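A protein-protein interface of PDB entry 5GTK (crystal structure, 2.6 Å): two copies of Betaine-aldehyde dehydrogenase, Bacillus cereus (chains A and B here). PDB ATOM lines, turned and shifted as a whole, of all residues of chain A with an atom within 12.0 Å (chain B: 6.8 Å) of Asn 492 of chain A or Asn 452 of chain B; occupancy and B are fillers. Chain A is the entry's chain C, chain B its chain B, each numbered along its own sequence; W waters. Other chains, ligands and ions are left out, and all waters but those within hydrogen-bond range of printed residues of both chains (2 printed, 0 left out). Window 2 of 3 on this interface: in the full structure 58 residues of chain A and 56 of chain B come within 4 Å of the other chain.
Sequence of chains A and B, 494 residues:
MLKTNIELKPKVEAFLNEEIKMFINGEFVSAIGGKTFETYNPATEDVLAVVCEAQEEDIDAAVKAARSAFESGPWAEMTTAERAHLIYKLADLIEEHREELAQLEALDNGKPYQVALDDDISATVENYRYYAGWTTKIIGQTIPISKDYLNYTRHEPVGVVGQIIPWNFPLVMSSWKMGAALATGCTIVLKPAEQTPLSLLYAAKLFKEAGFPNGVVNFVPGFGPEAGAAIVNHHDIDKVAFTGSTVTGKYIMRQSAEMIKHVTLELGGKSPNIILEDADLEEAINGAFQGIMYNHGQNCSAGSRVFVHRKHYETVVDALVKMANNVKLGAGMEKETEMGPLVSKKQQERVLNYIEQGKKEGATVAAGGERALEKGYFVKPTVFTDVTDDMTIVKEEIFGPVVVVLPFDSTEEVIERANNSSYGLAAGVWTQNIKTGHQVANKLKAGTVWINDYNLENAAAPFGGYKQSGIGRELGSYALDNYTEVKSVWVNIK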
ATOM      1  N   ILE A 143       5.593 -36.055 -11.110  1.00  0.00           N
ATOM      2  CA  ILE A 143       6.068 -36.417  -9.803  1.00  0.00           C
ATOM      3  C   ILE A 143       6.021 -35.337  -8.753  1.00  0.00           C
ATOM      4  O   ILE A 143       6.593 -34.337  -8.903  1.00  0.00           O
ATOM      5  CB  ILE A 143       7.494 -37.017  -9.901  1.00  0.00           C
ATOM      6  CG1 ILE A 143       7.529 -38.020 -11.000  1.00  0.00           C
ATOM      7  CG2 ILE A 143       7.918 -37.702  -8.629  1.00  0.00           C
ATOM      8  CD1 ILE A 143       8.713 -37.938 -11.904  1.00  0.00           C
ATOM      9  N   ILE A 145       7.318 -33.741  -5.701  1.00  0.00           N
ATOM     10  CA  ILE A 145       8.504 -33.731  -4.872  1.00  0.00           C
ATOM     11  C   ILE A 145       8.419 -32.521  -3.952  1.00  0.00           C
ATOM     12  O   ILE A 145       8.504 -32.632  -2.717  1.00  0.00           O
ATOM     13  CB  ILE A 145       9.745 -33.713  -5.755  1.00  0.00           C
ATOM     14  CG1 ILE A 145       9.701 -34.952  -6.660  1.00  0.00           C
ATOM     15  CG2 ILE A 145      11.010 -33.727  -4.918  1.00  0.00           C
ATOM     16  CD1 ILE A 145      10.839 -35.114  -7.652  1.00  0.00           C
ATOM     17  N   SER A 146       8.228 -31.368  -4.560  1.00  0.00           N
ATOM     18  CA  SER A 146       8.278 -30.130  -3.859  1.00  0.00           C
ATOM     19  C   SER A 146       7.323 -29.141  -4.558  1.00  0.00           C
ATOM     20  O   SER A 146       7.099 -29.198  -5.779  1.00  0.00           O
ATOM     21  CB  SER A 146       9.742 -29.674  -3.853  1.00  0.00           C
ATOM     22  OG  SER A 146       9.867 -28.279  -3.869  1.00  0.00           O
ATOM     23  N   LYS A 147       6.746 -28.256  -3.757  1.00  0.00           N
ATOM     24  CA  LYS A 147       5.949 -27.145  -4.275  1.00  0.00           C
ATOM     25  C   LYS A 147       6.759 -26.186  -5.192  1.00  0.00           C
ATOM     26  O   LYS A 147       6.155 -25.449  -5.957  1.00  0.00           O
ATOM     27  CB  LYS A 147       5.333 -26.342  -3.118  1.00  0.00           C
ATOM     28  CG  LYS A 147       6.327 -25.357  -2.499  1.00  0.00           C
ATOM     29  CD  LYS A 147       5.824 -24.717  -1.195  1.00  0.00           C
ATOM     30  CE  LYS A 147       6.727 -23.574  -0.738  1.00  0.00           C
ATOM     31  NZ  LYS A 147       8.018 -24.108  -0.230  1.00  0.00           N
ATOM     32  N   ASP A 148       8.095 -26.173  -5.055  1.00  0.00           N
ATOM     33  CA  ASP A 148       9.009 -25.282  -5.828  1.00  0.00           C
ATOM     34  C   ASP A 148       9.317 -25.755  -7.248  1.00  0.00           C
ATOM     35  O   ASP A 148       9.894 -25.004  -7.995  1.00  0.00           O
ATOM     36  CB  ASP A 148      10.372 -25.109  -5.130  1.00  0.00           C
ATOM     37  CG  ASP A 148      10.284 -24.421  -3.741  1.00  0.00           C
ATOM     38  OD1 ASP A 148       9.332 -23.605  -3.487  1.00  0.00           O
ATOM     39  OD2 ASP A 148      11.206 -24.695  -2.918  1.00  0.00           O
ATOM     40  N   TYR A 149       8.956 -26.997  -7.598  1.00  0.00           N
ATOM     41  CA  TYR A 149       9.183 -27.575  -8.929  1.00  0.00           C
ATOM     42  C   TYR A 149       7.969 -28.282  -9.497  1.00  0.00           C
ATOM     43  O   TYR A 149       7.201 -28.901  -8.784  1.00  0.00           O
ATOM     44  CB  TYR A 149      10.341 -28.583  -8.890  1.00  0.00           C
ATOM     45  CG  TYR A 149      11.566 -27.952  -8.386  1.00  0.00           C
ATOM     46  CD1 TYR A 149      12.344 -27.179  -9.231  1.00  0.00           C
ATOM     47  CD2 TYR A 149      11.931 -28.055  -7.046  1.00  0.00           C
ATOM     48  CE1 TYR A 149      13.483 -26.531  -8.770  1.00  0.00           C
ATOM     49  CE2 TYR A 149      13.078 -27.409  -6.557  1.00  0.00           C
ATOM     50  CZ  TYR A 149      13.835 -26.638  -7.429  1.00  0.00           C
ATOM     51  OH  TYR A 149      14.955 -25.990  -7.010  1.00  0.00           O
ATOM     52  N   LEU A 150       7.830 -28.175 -10.808  1.00  0.00           N
ATOM     53  CA  LEU A 150       7.109 -29.166 -11.603  1.00  0.00           C
ATOM     54  C   LEU A 150       8.130 -30.226 -12.103  1.00  0.00           C
ATOM     55  O   LEU A 150       9.142 -29.879 -12.732  1.00  0.00           O
ATOM     56  CB  LEU A 150       6.354 -28.501 -12.762  1.00  0.00           C
ATOM     57  CG  LEU A 150       5.900 -29.387 -13.935  1.00  0.00           C
ATOM     58  CD1 LEU A 150       4.850 -30.374 -13.449  1.00  0.00           C
ATOM     59  CD2 LEU A 150       5.358 -28.562 -15.108  1.00  0.00           C
ATOM     60  N   ASN A 151       7.880 -31.491 -11.751  1.00  0.00           N
ATOM     61  CA  ASN A 151       8.655 -32.613 -12.203  1.00  0.00           C
ATOM     62  C   ASN A 151       7.785 -33.459 -13.084  1.00  0.00           C
ATOM     63  O   ASN A 151       6.714 -33.858 -12.661  1.00  0.00           O
ATOM     64  CB  ASN A 151       9.069 -33.489 -11.046  1.00  0.00           C
ATOM     65  CG  ASN A 151      10.086 -32.838 -10.178  1.00  0.00           C
ATOM     66  OD1 ASN A 151       9.731 -32.186  -9.187  1.00  0.00           O
ATOM     67  ND2 ASN A 151      11.365 -32.987 -10.536  1.00  0.00           N
ATOM     68  N   TYR A 152       8.270 -33.753 -14.291  1.00  0.00           N
ATOM     69  CA  TYR A 152       7.608 -34.672 -15.163  1.00  0.00           C
ATOM     70  C   TYR A 152       8.628 -35.438 -16.031  1.00  0.00           C
ATOM     71  O   TYR A 152       9.758 -34.949 -16.253  1.00  0.00           O
ATOM     72  CB  TYR A 152       6.546 -33.946 -16.013  1.00  0.00           C
ATOM     73  CG  TYR A 152       7.056 -33.017 -17.091  1.00  0.00           C
ATOM     74  CD1 TYR A 152       7.284 -33.469 -18.381  1.00  0.00           C
ATOM     75  CD2 TYR A 152       7.252 -31.661 -16.830  1.00  0.00           C
ATOM     76  CE1 TYR A 152       7.733 -32.612 -19.381  1.00  0.00           C
ATOM     77  CE2 TYR A 152       7.686 -30.786 -17.818  1.00  0.00           C
ATOM     78  CZ  TYR A 152       7.940 -31.268 -19.094  1.00  0.00           C
ATOM     79  OH  TYR A 152       8.384 -30.393 -20.055  1.00  0.00           O
ATOM     80  N   SER A 488      13.661 -36.814 -17.776  1.00  0.00           N
ATOM     81  CA  SER A 488      13.183 -36.179 -16.553  1.00  0.00           C
ATOM     82  C   SER A 488      13.390 -34.667 -16.650  1.00  0.00           C
ATOM     83  O   SER A 488      14.524 -34.207 -16.793  1.00  0.00           O
ATOM     84  CB  SER A 488      13.944 -36.702 -15.334  1.00  0.00           C
ATOM     85  OG  SER A 488      13.490 -36.056 -14.144  1.00  0.00           O
ATOM     86  N   VAL A 489      12.296 -33.916 -16.551  1.00  0.00           N
ATOM     87  CA  VAL A 489      12.314 -32.474 -16.723  1.00  0.00           C
ATOM     88  C   VAL A 489      11.936 -31.857 -15.400  1.00  0.00           C
ATOM     89  O   VAL A 489      10.949 -32.264 -14.778  1.00  0.00           O
ATOM     90  CB  VAL A 489      11.303 -32.015 -17.814  1.00  0.00           C
ATOM     91  CG1 VAL A 489      11.391 -30.520 -18.044  1.00  0.00           C
ATOM     92  CG2 VAL A 489      11.568 -32.755 -19.122  1.00  0.00           C
ATOM     93  N   TRP A 490      12.734 -30.902 -14.966  1.00  0.00           N
ATOM     94  CA  TRP A 490      12.474 -30.134 -13.764  1.00  0.00           C
ATOM     95  C   TRP A 490      12.228 -28.682 -14.158  1.00  0.00           C
ATOM     96  O   TRP A 490      13.074 -28.047 -14.775  1.00  0.00           O
ATOM     97  CB  TRP A 490      13.684 -30.121 -12.869  1.00  0.00           C
ATOM     98  CG  TRP A 490      14.118 -31.413 -12.302  1.00  0.00           C
ATOM     99  CD1 TRP A 490      14.611 -32.528 -12.979  1.00  0.00           C
ATOM    100  CD2 TRP A 490      14.226 -31.707 -10.915  1.00  0.00           C
ATOM    101  NE1 TRP A 490      14.981 -33.503 -12.067  1.00  0.00           N
ATOM    102  CE2 TRP A 490      14.766 -33.015 -10.799  1.00  0.00           C
ATOM    103  CE3 TRP A 490      13.903 -30.994  -9.750  1.00  0.00           C
ATOM    104  CZ2 TRP A 490      14.972 -33.617  -9.559  1.00  0.00           C
ATOM    105  CZ3 TRP A 490      14.114 -31.566  -8.549  1.00  0.00           C
ATOM    106  CH2 TRP A 490      14.640 -32.882  -8.442  1.00  0.00           C
ATOM    107  N   VAL A 491      11.073 -28.173 -13.784  1.00  0.00           N
ATOM    108  CA  VAL A 491      10.690 -26.818 -14.046  1.00  0.00           C
ATOM    109  C   VAL A 491      10.595 -26.123 -12.679  1.00  0.00           C
ATOM    110  O   VAL A 491       9.668 -26.370 -11.885  1.00  0.00           O
ATOM    111  CB  VAL A 491       9.320 -26.752 -14.774  1.00  0.00           C
ATOM    112  CG1 VAL A 491       9.045 -25.330 -15.260  1.00  0.00           C
ATOM    113  CG2 VAL A 491       9.259 -27.772 -15.902  1.00  0.00           C
ATOM    114  N   ASN A 492      11.583 -25.266 -12.440  1.00  0.00           N
ATOM    115  CA  ASN A 492      11.609 -24.365 -11.303  1.00  0.00           C
ATOM    116  C   ASN A 492      10.425 -23.409 -11.445  1.00  0.00           C
ATOM    117  O   ASN A 492      10.306 -22.731 -12.454  1.00  0.00           O
ATOM    118  CB  ASN A 492      12.974 -23.641 -11.314  1.00  0.00           C
ATOM    119  CG  ASN A 492      13.148 -22.602 -10.188  1.00  0.00           C
ATOM    120  OD1 ASN A 492      12.250 -21.794  -9.860  1.00  0.00           O
ATOM    121  ND2 ASN A 492      14.323 -22.593  -9.633  1.00  0.00           N
ATOM    122  N   ILE A 493       9.530 -23.415 -10.456  1.00  0.00           N
ATOM    123  CA  ILE A 493       8.328 -22.559 -10.440  1.00  0.00           C
ATOM    124  C   ILE A 493       8.305 -21.763  -9.149  1.00  0.00           C
ATOM    125  O   ILE A 493       7.271 -21.335  -8.641  1.00  0.00           O
ATOM    126  CB  ILE A 493       7.022 -23.342 -10.675  1.00  0.00           C
ATOM    127  CG1 ILE A 493       6.817 -24.431  -9.631  1.00  0.00           C
ATOM    128  CG2 ILE A 493       7.042 -23.950 -12.067  1.00  0.00           C
ATOM    129  CD1 ILE A 493       5.462 -25.114  -9.686  1.00  0.00           C
ATOM    130  N   LYS A 494       9.490 -21.493  -8.661  1.00  0.00           N
ATOM    131  CA  LYS A 494       9.660 -20.827  -7.396  1.00  0.00           C
ATOM    132  C   LYS A 494       9.479 -19.321  -7.597  1.00  0.00           C
ATOM    133  O   LYS A 494       9.492 -18.765  -8.743  1.00  0.00           O
ATOM    134  CB  LYS A 494      11.065 -21.096  -6.906  1.00  0.00           C
ATOM    135  CG  LYS A 494      11.198 -21.177  -5.424  1.00  0.00           C
ATOM    136  CD  LYS A 494      12.678 -21.282  -5.050  1.00  0.00           C
ATOM    137  CE  LYS A 494      13.399 -22.450  -5.715  1.00  0.00           C
ATOM    138  NZ  LYS A 494      14.648 -22.726  -4.969  1.00  0.00           N
ATOM    139  OXT LYS A 494       9.324 -18.642  -6.572  1.00  0.00           O
ATOM    140  N   ASP B 278      16.369 -14.227 -22.997  1.00  0.00           N
ATOM    141  CA  ASP B 278      15.430 -13.818 -21.961  1.00  0.00           C
ATOM    142  C   ASP B 278      15.611 -14.551 -20.618  1.00  0.00           C
ATOM    143  O   ASP B 278      14.719 -14.519 -19.773  1.00  0.00           O
ATOM    144  CB  ASP B 278      13.986 -13.868 -22.460  1.00  0.00           C
ATOM    145  CG  ASP B 278      13.565 -15.235 -22.993  1.00  0.00           C
ATOM    146  OD1 ASP B 278      14.369 -16.181 -23.136  1.00  0.00           O
ATOM    147  OD2 ASP B 278      12.385 -15.345 -23.327  1.00  0.00           O
ATOM    148  N   ALA B 279      16.768 -15.153 -20.375  1.00  0.00           N
ATOM    149  CA  ALA B 279      17.067 -15.634 -19.016  1.00  0.00           C
ATOM    150  C   ALA B 279      16.966 -14.494 -18.003  1.00  0.00           C
ATOM    151  O   ALA B 279      17.246 -13.346 -18.324  1.00  0.00           O
ATOM    152  CB  ALA B 279      18.463 -16.243 -18.942  1.00  0.00           C
ATOM    153  N   ASP B 280      16.562 -14.835 -16.790  1.00  0.00           N
ATOM    154  CA  ASP B 280      16.953 -14.056 -15.623  1.00  0.00           C
ATOM    155  C   ASP B 280      18.458 -14.211 -15.392  1.00  0.00           C
ATOM    156  O   ASP B 280      18.936 -15.215 -14.859  1.00  0.00           O
ATOM    157  CB  ASP B 280      16.231 -14.487 -14.380  1.00  0.00           C
ATOM    158  CG  ASP B 280      16.380 -13.487 -13.288  1.00  0.00           C
ATOM    159  OD1 ASP B 280      17.439 -13.448 -12.626  1.00  0.00           O
ATOM    160  OD2 ASP B 280      15.443 -12.701 -13.113  1.00  0.00           O
ATOM    161  N   GLU B 283      20.095 -15.118 -11.869  1.00  0.00           N
ATOM    162  CA  GLU B 283      19.888 -16.516 -11.487  1.00  0.00           C
ATOM    163  C   GLU B 283      20.654 -17.526 -12.352  1.00  0.00           C
ATOM    164  O   GLU B 283      21.206 -18.492 -11.811  1.00  0.00           O
ATOM    165  CB  GLU B 283      18.401 -16.832 -11.415  1.00  0.00           C
ATOM    166  CG  GLU B 283      17.770 -16.327 -10.123  1.00  0.00           C
ATOM    167  CD  GLU B 283      16.255 -16.232 -10.182  1.00  0.00           C
ATOM    168  OE1 GLU B 283      15.666 -16.230 -11.302  1.00  0.00           O
ATOM    169  OE2 GLU B 283      15.644 -16.141  -9.090  1.00  0.00           O
ATOM    170  N   ALA B 284      20.692 -17.299 -13.667  1.00  0.00           N
ATOM    171  CA  ALA B 284      21.432 -18.165 -14.601  1.00  0.00           C
ATOM    172  C   ALA B 284      22.956 -18.155 -14.409  1.00  0.00           C
ATOM    173  O   ALA B 284      23.636 -19.168 -14.675  1.00  0.00           O
ATOM    174  CB  ALA B 284      21.087 -17.831 -16.057  1.00  0.00           C
ATOM    175  N   GLY B 428      20.925 -27.968 -18.945  1.00  0.00           N
ATOM    176  CA  GLY B 428      20.226 -26.862 -18.325  1.00  0.00           C
ATOM    177  C   GLY B 428      19.755 -25.881 -19.359  1.00  0.00           C
ATOM    178  O   GLY B 428      20.475 -25.643 -20.328  1.00  0.00           O
ATOM    179  N   VAL B 429      18.558 -25.311 -19.168  1.00  0.00           N
ATOM    180  CA  VAL B 429      18.104 -24.226 -20.029  1.00  0.00           C
ATOM    181  C   VAL B 429      17.475 -23.089 -19.216  1.00  0.00           C
ATOM    182  O   VAL B 429      16.572 -23.321 -18.391  1.00  0.00           O
ATOM    183  CB  VAL B 429      17.218 -24.744 -21.198  1.00  0.00           C
ATOM    184  CG1 VAL B 429      16.118 -25.625 -20.732  1.00  0.00           C
ATOM    185  CG2 VAL B 429      16.621 -23.593 -21.992  1.00  0.00           C
ATOM    186  N   TRP B 430      17.990 -21.866 -19.459  1.00  0.00           N
ATOM    187  CA  TRP B 430      17.576 -20.643 -18.750  1.00  0.00           C
ATOM    188  C   TRP B 430      16.833 -19.693 -19.691  1.00  0.00           C
ATOM    189  O   TRP B 430      17.410 -19.183 -20.662  1.00  0.00           O
ATOM    190  CB  TRP B 430      18.783 -19.968 -18.130  1.00  0.00           C
ATOM    191  CG  TRP B 430      19.478 -20.893 -17.165  1.00  0.00           C
ATOM    192  CD1 TRP B 430      20.331 -21.912 -17.468  1.00  0.00           C
ATOM    193  CD2 TRP B 430      19.321 -20.905 -15.762  1.00  0.00           C
ATOM    194  NE1 TRP B 430      20.718 -22.551 -16.333  1.00  0.00           N
ATOM    195  CE2 TRP B 430      20.126 -21.945 -15.263  1.00  0.00           C
ATOM    196  CE3 TRP B 430      18.610 -20.102 -14.858  1.00  0.00           C
ATOM    197  CZ2 TRP B 430      20.231 -22.221 -13.895  1.00  0.00           C
ATOM    198  CZ3 TRP B 430      18.710 -20.373 -13.483  1.00  0.00           C
ATOM    199  CH2 TRP B 430      19.507 -21.422 -13.020  1.00  0.00           C
ATOM    200  N   THR B 431      15.542 -19.519 -19.424  1.00  0.00           N
ATOM    201  CA  THR B 431      14.669 -18.734 -20.249  1.00  0.00           C
ATOM    202  C   THR B 431      13.451 -18.475 -19.421  1.00  0.00           C
ATOM    203  O   THR B 431      13.004 -19.365 -18.738  1.00  0.00           O
ATOM    204  CB  THR B 431      14.250 -19.463 -21.549  1.00  0.00           C
ATOM    205  OG1 THR B 431      13.331 -18.640 -22.263  1.00  0.00           O
ATOM    206  CG2 THR B 431      13.578 -20.861 -21.293  1.00  0.00           C
ATOM    207  N   GLN B 432      12.944 -17.246 -19.474  1.00  0.00           N
ATOM    208  CA  GLN B 432      11.699 -16.848 -18.782  1.00  0.00           C
ATOM    209  C   GLN B 432      10.450 -17.174 -19.573  1.00  0.00           C
ATOM    210  O   GLN B 432       9.375 -17.105 -19.013  1.00  0.00           O
ATOM    211  CB  GLN B 432      11.690 -15.353 -18.435  1.00  0.00           C
ATOM    212  CG  GLN B 432      12.684 -14.971 -17.362  1.00  0.00           C
ATOM    213  CD  GLN B 432      12.307 -15.493 -15.969  1.00  0.00           C
ATOM    214  OE1 GLN B 432      12.961 -16.403 -15.411  1.00  0.00           O
ATOM    215  NE2 GLN B 432      11.259 -14.919 -15.396  1.00  0.00           N
ATOM    216  N   ASN B 433      10.581 -17.557 -20.837  1.00  0.00           N
ATOM    217  CA  ASN B 433       9.427 -17.755 -21.691  1.00  0.00           C
ATOM    218  C   ASN B 433       8.885 -19.194 -21.619  1.00  0.00           C
ATOM    219  O   ASN B 433       9.645 -20.154 -21.728  1.00  0.00           O
ATOM    220  CB  ASN B 433       9.785 -17.378 -23.143  1.00  0.00           C
ATOM    221  CG  ASN B 433       8.580 -17.388 -24.052  1.00  0.00           C
ATOM    222  OD1 ASN B 433       7.936 -16.377 -24.223  1.00  0.00           O
ATOM    223  ND2 ASN B 433       8.214 -18.538 -24.538  1.00  0.00           N
ATOM    224  N   GLY B 437      10.955 -22.579 -23.095  1.00  0.00           N
ATOM    225  CA  GLY B 437      11.466 -23.531 -22.072  1.00  0.00           C
ATOM    226  C   GLY B 437      11.221 -24.997 -22.433  1.00  0.00           C
ATOM    227  O   GLY B 437      12.124 -25.788 -22.537  1.00  0.00           O
ATOM    228  N   TRP B 450      16.825 -29.498 -16.741  1.00  0.00           N
ATOM    229  CA  TRP B 450      16.489 -28.524 -15.763  1.00  0.00           C
ATOM    230  C   TRP B 450      16.141 -27.220 -16.491  1.00  0.00           C
ATOM    231  O   TRP B 450      16.873 -26.760 -17.300  1.00  0.00           O
ATOM    232  CB  TRP B 450      17.654 -28.301 -14.832  1.00  0.00           C
ATOM    233  CG  TRP B 450      18.081 -29.476 -14.043  1.00  0.00           C
ATOM    234  CD1 TRP B 450      17.422 -30.038 -13.049  1.00  0.00           C
ATOM    235  CD2 TRP B 450      19.310 -30.211 -14.161  1.00  0.00           C
ATOM    236  NE1 TRP B 450      18.087 -31.065 -12.563  1.00  0.00           N
ATOM    237  CE2 TRP B 450      19.267 -31.200 -13.215  1.00  0.00           C
ATOM    238  CE3 TRP B 450      20.418 -30.133 -14.992  1.00  0.00           C
ATOM    239  CZ2 TRP B 450      20.299 -32.100 -13.053  1.00  0.00           C
ATOM    240  CZ3 TRP B 450      21.406 -30.996 -14.825  1.00  0.00           C
ATOM    241  CH2 TRP B 450      21.369 -31.957 -13.859  1.00  0.00           C
ATOM    242  N   ILE B 451      14.980 -26.673 -16.222  1.00  0.00           N
ATOM    243  CA  ILE B 451      14.544 -25.424 -16.804  1.00  0.00           C
ATOM    244  C   ILE B 451      14.616 -24.419 -15.678  1.00  0.00           C
ATOM    245  O   ILE B 451      13.840 -24.430 -14.799  1.00  0.00           O
ATOM    246  CB  ILE B 451      13.130 -25.462 -17.443  1.00  0.00           C
ATOM    247  CG1 ILE B 451      12.988 -26.555 -18.478  1.00  0.00           C
ATOM    248  CG2 ILE B 451      12.825 -24.142 -18.098  1.00  0.00           C
ATOM    249  CD1 ILE B 451      11.592 -26.815 -18.981  1.00  0.00           C
ATOM    250  N   ASN B 452      15.605 -23.561 -15.743  1.00  0.00           N
ATOM    251  CA  ASN B 452      15.880 -22.520 -14.771  1.00  0.00           C
ATOM    252  C   ASN B 452      16.411 -23.017 -13.466  1.00  0.00           C
ATOM    253  O   ASN B 452      16.108 -22.507 -12.475  1.00  0.00           O
ATOM    254  CB  ASN B 452      14.750 -21.505 -14.583  1.00  0.00           C
ATOM    255  CG  ASN B 452      14.393 -20.790 -15.844  1.00  0.00           C
ATOM    256  OD1 ASN B 452      15.206 -20.324 -16.479  1.00  0.00           O
ATOM    257  ND2 ASN B 452      13.181 -20.782 -16.198  1.00  0.00           N
ATOM    258  N   ASP B 453      17.253 -24.005 -13.527  1.00  0.00           N
ATOM    259  CA  ASP B 453      17.900 -24.549 -12.389  1.00  0.00           C
ATOM    260  C   ASP B 453      18.955 -25.448 -12.924  1.00  0.00           C
ATOM    261  O   ASP B 453      19.138 -25.460 -14.061  1.00  0.00           O
ATOM    262  CB  ASP B 453      16.923 -25.239 -11.478  1.00  0.00           C
ATOM    263  CG  ASP B 453      17.184 -24.941 -10.083  1.00  0.00           C
ATOM    264  OD1 ASP B 453      18.274 -25.029  -9.690  1.00  0.00           O
ATOM    265  OD2 ASP B 453      16.321 -24.590  -9.360  1.00  0.00           O
ATOM    266  N   TYR B 454      19.651 -26.156 -12.090  1.00  0.00           N
ATOM    267  CA  TYR B 454      20.680 -27.046 -12.509  1.00  0.00           C
ATOM    268  C   TYR B 454      21.086 -27.911 -11.360  1.00  0.00           C
ATOM    269  O   TYR B 454      21.067 -27.490 -10.240  1.00  0.00           O
ATOM    270  CB  TYR B 454      21.920 -26.293 -13.081  1.00  0.00           C
ATOM    271  CG  TYR B 454      22.700 -27.146 -14.033  1.00  0.00           C
ATOM    272  CD1 TYR B 454      23.728 -27.918 -13.616  1.00  0.00           C
ATOM    273  CD2 TYR B 454      22.312 -27.261 -15.313  1.00  0.00           C
ATOM    274  CE1 TYR B 454      24.363 -28.735 -14.459  1.00  0.00           C
ATOM    275  CE2 TYR B 454      22.959 -28.056 -16.165  1.00  0.00           C
ATOM    276  CZ  TYR B 454      23.974 -28.789 -15.739  1.00  0.00           C
ATOM    277  OH  TYR B 454      24.543 -29.578 -16.647  1.00  0.00           O
ATOM    278  N   LEU B 456      19.754 -30.583  -9.851  1.00  0.00           N
ATOM    279  CA  LEU B 456      18.810 -31.095  -8.873  1.00  0.00           C
ATOM    280  C   LEU B 456      18.605 -32.620  -9.028  1.00  0.00           C
ATOM    281  O   LEU B 456      18.407 -33.148 -10.140  1.00  0.00           O
ATOM    282  CB  LEU B 456      17.507 -30.324  -8.987  1.00  0.00           C
ATOM    283  CG  LEU B 456      17.671 -28.792  -8.807  1.00  0.00           C
ATOM    284  CD1 LEU B 456      16.374 -28.070  -9.196  1.00  0.00           C
ATOM    285  CD2 LEU B 456      18.113 -28.385  -7.403  1.00  0.00           C
HETATM  286  O   HOH W   1      15.235 -20.019 -11.471  1.00  0.00           O
HETATM  287  O   HOH W   2      11.505 -22.621 -15.072  1.00  0.00           O
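No position is printed for both chains. Of the 10 pairs that touch across the chains among the printed residues, none has its exchanged pair printed and touching as well.
The backbone NH (N) of Ile 451 of chain B lies within hydrogen-bond range of the backbone carbonyl oxygen (O) of Trp 490 of chain A (2.8 Å). N of Asn 492 of chain A lies within hydrogen-bond range of O of Ile 451 of chain B (3.4 Å). The backbone carbonyl oxygen of Asn 452 of chain B lies within hydrogen-bond range of the side-chain amide nitrogen of Asn 492 of chain A (3.4 Å). OD2 of Asp 453 of chain B lies within hydrogen-bond range of OH of Tyr 149 of chain A (3.1 Å). OD2 of Asp 453 of chain B sits at hydrogen-bond distance from ND2 of Asn 492 of chain A (2.8 Å).
Of the printed residues of chain B, Tyr 149 of chain A touches Asp 453 (3.1 Å) and Leu 456 (3.3 Å). Of the printed residues of chain B, Val 489 of chain A touches Ile 451. Printed residues of chain B within 4 Å of Val 491 of chain A: Ile 451 (3.98 Å). Printed residues of chain B within 4 Å of Asn 492 of chain A: Ile 451, Asn 452 and Asp 453. No residue of chain A comes within 4 Å of Val 429 of chain B. No residue of chain A comes within 4 Å of Trp 430 of chain B. Thr 431 of chain B touches none of the printed residues of chain A. Gln 432 of chain B touches none of the printed residues of chain A. Asn 452 of chain B touches just one residue of chain A: Asn 492. Of chain A, only Tyr 149 (3.1 Å) and Asn 492 (2.8 Å) come within 4 Å of Asp 453 of chain B. The nearest residue of chain A that does not touch Asn 452 of chain B is Trp 490 of chain A (5.2 Å).
N of Val 429 of chain B is in hydrogen-bond range of O of Trp 450 of chain B (2.9 Å). The side-chain amide nitrogen of Asn 452 of chain B sits at hydrogen-bond distance from the backbone carbonyl oxygen of Thr 431 of chain B (2.9 Å). NE1 of Trp 450 of chain B lies within hydrogen-bond range of O of Leu 456 of chain B (3.2 Å). The backbone carbonyl oxygen (O) of Leu 150 of chain A sits at hydrogen-bond distance from the backbone NH (N) of Val 491 of chain A. N of Val 489 of chain A lies within hydrogen-bond range of O of Tyr 152 of chain A, 2.8 Å away. The side-chain amide oxygen of Asn 492 of chain A is in hydrogen-bond range of the backbone NH of Lys 494 of chain A (3.0 Å).
Leu 456 of chain B touches Tyr 149 of chain A (CD1 to CE1, 3.3 Å). Val 489 of chain A touches Ile 451 of chain B. CA of Trp 450 of chain B touches O of Trp 490 of chain A, 3.6 Å away. Leu 456 of chain B touches Trp 490 of chain A. Ile 451 of chain B touches Val 491 of chain A (CD1 to CG2, 3.98 Å).
Hydrophobic or aromatic side chains of chain B within 4 Å of the printed part of chain A: Trp 450, Ile 451 and Leu 456. Hydrophobic or aromatic side chains of chain A within 4 Å of the printed part of chain B: Tyr 149, Val 489, Trp 490 and Val 491. Among the printed residues, 10 pairs touch across the chains.
Water W2 lies within hydrogen-bond range of the side-chain amide nitrogen of Asn 452 of chain B (2.7 Å), the backbone carbonyl oxygen of Asn 492 of chain A (2.9 Å) and the backbone carbonyl oxygen of Ile 451 of chain B (3.0 Å). Water W1 bridges the backbone carbonyl oxygen of Asn 452 of chain B and the side-chain amide nitrogen of Asn 492 of chain A.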
